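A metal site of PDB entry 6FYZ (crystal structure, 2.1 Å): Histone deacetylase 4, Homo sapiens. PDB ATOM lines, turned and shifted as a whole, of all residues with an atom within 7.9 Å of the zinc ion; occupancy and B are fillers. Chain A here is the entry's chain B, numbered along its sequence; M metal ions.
Within 4 Å of the zinc ion: Cys 23, Cys 25, His 31 and Cys 107.
The zinc ion is bound by NE2 of His 31, 2.1 Å away.
The side-chain sulfur (SG) of Cys 25 is bound to the zinc ion, at 2.1 Å.
The zinc ion is bound by the side-chain sulfur (SG) of Cys 107.
SG of Cys 23 binds the zinc ion (2.4 Å).
The zinc ion has four donor atoms within binding distance.
SG of Cys 25 sits close to N of Ser 27 (3.7 Å).
The backbone NH (N) of Gly 109 lies close to the side-chain sulfur (SG) of Cys 107 (3.7 Å).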
ATOM      1  N   GLN A  22      14.834 -19.243 -15.026  1.00  0.00           N
ATOM      2  CA  GLN A  22      15.469 -19.816 -16.216  1.00  0.00           C
ATOM      3  C   GLN A  22      16.557 -18.899 -16.649  1.00  0.00           C
ATOM      4  O   GLN A  22      16.380 -17.677 -16.644  1.00  0.00           O
ATOM      5  CB  GLN A  22      14.499 -19.903 -17.400  1.00  0.00           C
ATOM      6  CG  GLN A  22      13.707 -21.163 -17.513  1.00  0.00           C
ATOM      7  CD  GLN A  22      14.469 -22.313 -18.164  1.00  0.00           C
ATOM      8  OE1 GLN A  22      15.112 -23.105 -17.470  1.00  0.00           O
ATOM      9  NE2 GLN A  22      14.342 -22.433 -19.469  1.00  0.00           N
ATOM     10  N   CYS A  23      17.674 -19.471 -17.081  1.00  0.00           N
ATOM     11  CA  CYS A  23      18.655 -18.659 -17.760  1.00  0.00           C
ATOM     12  C   CYS A  23      18.051 -18.094 -19.048  1.00  0.00           C
ATOM     13  O   CYS A  23      17.279 -18.775 -19.719  1.00  0.00           O
ATOM     14  CB  CYS A  23      19.914 -19.434 -18.080  1.00  0.00           C
ATOM     15  SG  CYS A  23      21.216 -18.256 -18.416  1.00  0.00           S
ATOM     16  N   THR A  24      18.409 -16.864 -19.378  1.00  0.00           N
ATOM     17  CA  THR A  24      17.926 -16.228 -20.607  1.00  0.00           C
ATOM     18  C   THR A  24      18.468 -16.897 -21.880  1.00  0.00           C
ATOM     19  O   THR A  24      17.877 -16.713 -22.949  1.00  0.00           O
ATOM     20  CB  THR A  24      18.213 -14.711 -20.625  1.00  0.00           C
ATOM     21  OG1 THR A  24      19.580 -14.472 -20.283  1.00  0.00           O
ATOM     22  CG2 THR A  24      17.298 -13.990 -19.625  1.00  0.00           C
ATOM     23  N   CYS A  25      19.572 -17.643 -21.786  1.00  0.00           N
ATOM     24  CA  CYS A  25      20.015 -18.531 -22.884  1.00  0.00           C
ATOM     25  C   CYS A  25      18.967 -19.636 -23.193  1.00  0.00           C
ATOM     26  O   CYS A  25      18.817 -20.017 -24.344  1.00  0.00           O
ATOM     27  CB  CYS A  25      21.423 -19.133 -22.639  1.00  0.00           C
ATOM     28  SG  CYS A  25      21.637 -20.460 -21.396  1.00  0.00           S
ATOM     29  N   GLY A  26      18.247 -20.102 -22.175  1.00  0.00           N
ATOM     30  CA  GLY A  26      17.185 -21.114 -22.343  1.00  0.00           C
ATOM     31  C   GLY A  26      17.682 -22.522 -22.667  1.00  0.00           C
ATOM     32  O   GLY A  26      16.937 -23.315 -23.229  1.00  0.00           O
ATOM     33  N   SER A  27      18.923 -22.821 -22.267  1.00  0.00           N
ATOM     34  CA  SER A  27      19.596 -24.080 -22.595  1.00  0.00           C
ATOM     35  C   SER A  27      19.534 -25.092 -21.452  1.00  0.00           C
ATOM     36  O   SER A  27      19.984 -24.806 -20.345  1.00  0.00           O
ATOM     37  CB  SER A  27      21.069 -23.812 -22.932  1.00  0.00           C
ATOM     38  OG  SER A  27      21.801 -25.022 -23.058  1.00  0.00           O
ATOM     39  N   SER A  28      19.004 -26.276 -21.734  1.00  0.00           N
ATOM     40  CA  SER A  28      19.032 -27.401 -20.799  1.00  0.00           C
ATOM     41  C   SER A  28      20.450 -27.933 -20.543  1.00  0.00           C
ATOM     42  O   SER A  28      20.776 -28.329 -19.417  1.00  0.00           O
ATOM     43  CB  SER A  28      18.158 -28.552 -21.325  1.00  0.00           C
ATOM     44  OG  SER A  28      16.864 -28.081 -21.632  1.00  0.00           O
ATOM     45  N   SER A  30      23.643 -26.592 -20.498  1.00  0.00           N
ATOM     46  CA  SER A  30      24.493 -25.871 -19.552  1.00  0.00           C
ATOM     47  C   SER A  30      23.844 -25.684 -18.169  1.00  0.00           C
ATOM     48  O   SER A  30      24.542 -25.375 -17.196  1.00  0.00           O
ATOM     49  CB  SER A  30      24.934 -24.532 -20.154  1.00  0.00           C
ATOM     50  OG  SER A  30      24.081 -24.154 -21.229  1.00  0.00           O
ATOM     51  N   HIS A  31      22.525 -25.881 -18.082  1.00  0.00           N
ATOM     52  CA  HIS A  31      21.767 -25.701 -16.845  1.00  0.00           C
ATOM     53  C   HIS A  31      20.884 -26.917 -16.570  1.00  0.00           C
ATOM     54  O   HIS A  31      19.740 -26.980 -17.028  1.00  0.00           O
ATOM     55  CB  HIS A  31      20.958 -24.411 -16.949  1.00  0.00           C
ATOM     56  CG  HIS A  31      21.744 -23.282 -17.526  1.00  0.00           C
ATOM     57  ND1 HIS A  31      22.882 -22.779 -16.923  1.00  0.00           N
ATOM     58  CD2 HIS A  31      21.608 -22.596 -18.687  1.00  0.00           C
ATOM     59  CE1 HIS A  31      23.383 -21.816 -17.665  1.00  0.00           C
ATOM     60  NE2 HIS A  31      22.632 -21.689 -18.744  1.00  0.00           N
ATOM     61  N   LEU A 105      27.824 -15.023 -17.179  1.00  0.00           N
ATOM     62  CA  LEU A 105      28.256 -16.390 -17.512  1.00  0.00           C
ATOM     63  C   LEU A 105      28.690 -16.459 -18.989  1.00  0.00           C
ATOM     64  O   LEU A 105      28.463 -15.503 -19.750  1.00  0.00           O
ATOM     65  CB  LEU A 105      27.106 -17.371 -17.276  1.00  0.00           C
ATOM     66  CG  LEU A 105      26.459 -17.424 -15.887  1.00  0.00           C
ATOM     67  CD1 LEU A 105      25.427 -18.550 -15.842  1.00  0.00           C
ATOM     68  CD2 LEU A 105      27.495 -17.592 -14.776  1.00  0.00           C
ATOM     69  N   PRO A 106      29.316 -17.586 -19.413  1.00  0.00           N
ATOM     70  CA  PRO A 106      29.606 -17.798 -20.848  1.00  0.00           C
ATOM     71  C   PRO A 106      28.375 -17.772 -21.776  1.00  0.00           C
ATOM     72  O   PRO A 106      28.480 -17.323 -22.925  1.00  0.00           O
ATOM     73  CB  PRO A 106      30.283 -19.191 -20.887  1.00  0.00           C
ATOM     74  CG  PRO A 106      30.104 -19.773 -19.514  1.00  0.00           C
ATOM     75  CD  PRO A 106      29.994 -18.602 -18.588  1.00  0.00           C
ATOM     76  N   CYS A 107      27.227 -18.238 -21.277  1.00  0.00           N
ATOM     77  CA  CYS A 107      25.976 -18.228 -22.045  1.00  0.00           C
ATOM     78  C   CYS A 107      25.301 -16.843 -22.176  1.00  0.00           C
ATOM     79  O   CYS A 107      24.269 -16.710 -22.834  1.00  0.00           O
ATOM     80  CB  CYS A 107      24.992 -19.224 -21.420  1.00  0.00           C
ATOM     81  SG  CYS A 107      24.638 -18.925 -19.655  1.00  0.00           S
ATOM     82  N   GLY A 108      25.876 -15.811 -21.541  1.00  0.00           N
ATOM     83  CA  GLY A 108      25.285 -14.475 -21.525  1.00  0.00           C
ATOM     84  C   GLY A 108      24.269 -14.282 -20.408  1.00  0.00           C
ATOM     85  O   GLY A 108      23.601 -13.253 -20.355  1.00  0.00           O
ATOM     86  N   GLY A 109      24.159 -15.274 -19.530  1.00  0.00           N
ATOM     87  CA  GLY A 109      23.235 -15.216 -18.406  1.00  0.00           C
ATOM     88  C   GLY A 109      23.880 -14.596 -17.184  1.00  0.00           C
ATOM     89  O   GLY A 109      25.059 -14.239 -17.194  1.00  0.00           O
ATOM     90  N   VAL A 110      23.078 -14.458 -16.133  1.00  0.00           N
ATOM     91  CA  VAL A 110      23.528 -14.000 -14.829  1.00  0.00           C
ATOM     92  C   VAL A 110      23.534 -15.227 -13.916  1.00  0.00           C
ATOM     93  O   VAL A 110      22.869 -16.232 -14.211  1.00  0.00           O
ATOM     94  CB  VAL A 110      22.588 -12.876 -14.308  1.00  0.00           C
ATOM     95  CG1 VAL A 110      23.104 -12.281 -12.997  1.00  0.00           C
ATOM     96  CG2 VAL A 110      22.444 -11.794 -15.368  1.00  0.00           C
ATOM     97  N   SER A 114      29.379 -20.835 -13.643  1.00  0.00           N
ATOM     98  CA  SER A 114      29.125 -21.469 -14.966  1.00  0.00           C
ATOM     99  C   SER A 114      27.731 -22.102 -15.204  1.00  0.00           C
ATOM    100  O   SER A 114      27.124 -21.870 -16.251  1.00  0.00           O
ATOM    101  CB  SER A 114      30.220 -22.531 -15.225  1.00  0.00           C
ATOM    102  OG  SER A 114      30.009 -23.226 -16.444  1.00  0.00           O
ATOM    103  N   ASP A 115      27.250 -22.886 -14.229  1.00  0.00           N
ATOM    104  CA  ASP A 115      26.001 -23.675 -14.384  1.00  0.00           C
ATOM    105  C   ASP A 115      24.837 -23.331 -13.404  1.00  0.00           C
ATOM    106  O   ASP A 115      23.732 -23.823 -13.621  1.00  0.00           O
ATOM    107  CB  ASP A 115      26.298 -25.192 -14.360  1.00  0.00           C
ATOM    108  CG  ASP A 115      27.327 -25.597 -13.297  1.00  0.00           C
ATOM    109  OD1 ASP A 115      27.289 -25.037 -12.187  1.00  0.00           O
ATOM    110  OD2 ASP A 115      28.168 -26.481 -13.587  1.00  0.00           O
ATOM    111  N   ILE A 117      22.145 -20.880 -12.271  1.00  0.00           N
ATOM    112  CA  ILE A 117      21.529 -19.761 -12.973  1.00  0.00           C
ATOM    113  C   ILE A 117      20.867 -18.774 -12.027  1.00  0.00           C
ATOM    114  O   ILE A 117      20.504 -19.149 -10.907  1.00  0.00           O
ATOM    115  CB  ILE A 117      20.510 -20.235 -14.043  1.00  0.00           C
ATOM    116  CG1 ILE A 117      19.173 -20.684 -13.442  1.00  0.00           C
ATOM    117  CG2 ILE A 117      21.124 -21.354 -14.876  1.00  0.00           C
ATOM    118  CD1 ILE A 117      18.081 -19.630 -13.500  1.00  0.00           C
ATOM    119  N   TRP A 118      20.706 -17.538 -12.488  1.00  0.00           N
ATOM    120  CA  TRP A 118      19.905 -16.541 -11.782  1.00  0.00           C
ATOM    121  C   TRP A 118      19.204 -15.582 -12.752  1.00  0.00           C
ATOM    122  O   TRP A 118      19.858 -14.759 -13.394  1.00  0.00           O
ATOM    123  CB  TRP A 118      20.755 -15.751 -10.795  1.00  0.00           C
ATOM    124  CG  TRP A 118      19.931 -14.904  -9.903  1.00  0.00           C
ATOM    125  CD1 TRP A 118      19.807 -13.560  -9.929  1.00  0.00           C
ATOM    126  CD2 TRP A 118      19.070 -15.369  -8.854  1.00  0.00           C
ATOM    127  NE1 TRP A 118      18.932 -13.145  -8.968  1.00  0.00           N
ATOM    128  CE2 TRP A 118      18.452 -14.234  -8.290  1.00  0.00           C
ATOM    129  CE3 TRP A 118      18.751 -16.638  -8.340  1.00  0.00           C
ATOM    130  CZ2 TRP A 118      17.552 -14.325  -7.226  1.00  0.00           C
ATOM    131  CZ3 TRP A 118      17.844 -16.732  -7.287  1.00  0.00           C
ATOM    132  CH2 TRP A 118      17.260 -15.580  -6.745  1.00  0.00           C
HETATM  133 ZN    ZN M   1      22.574 -19.830 -19.653  1.00  0.00          ZN
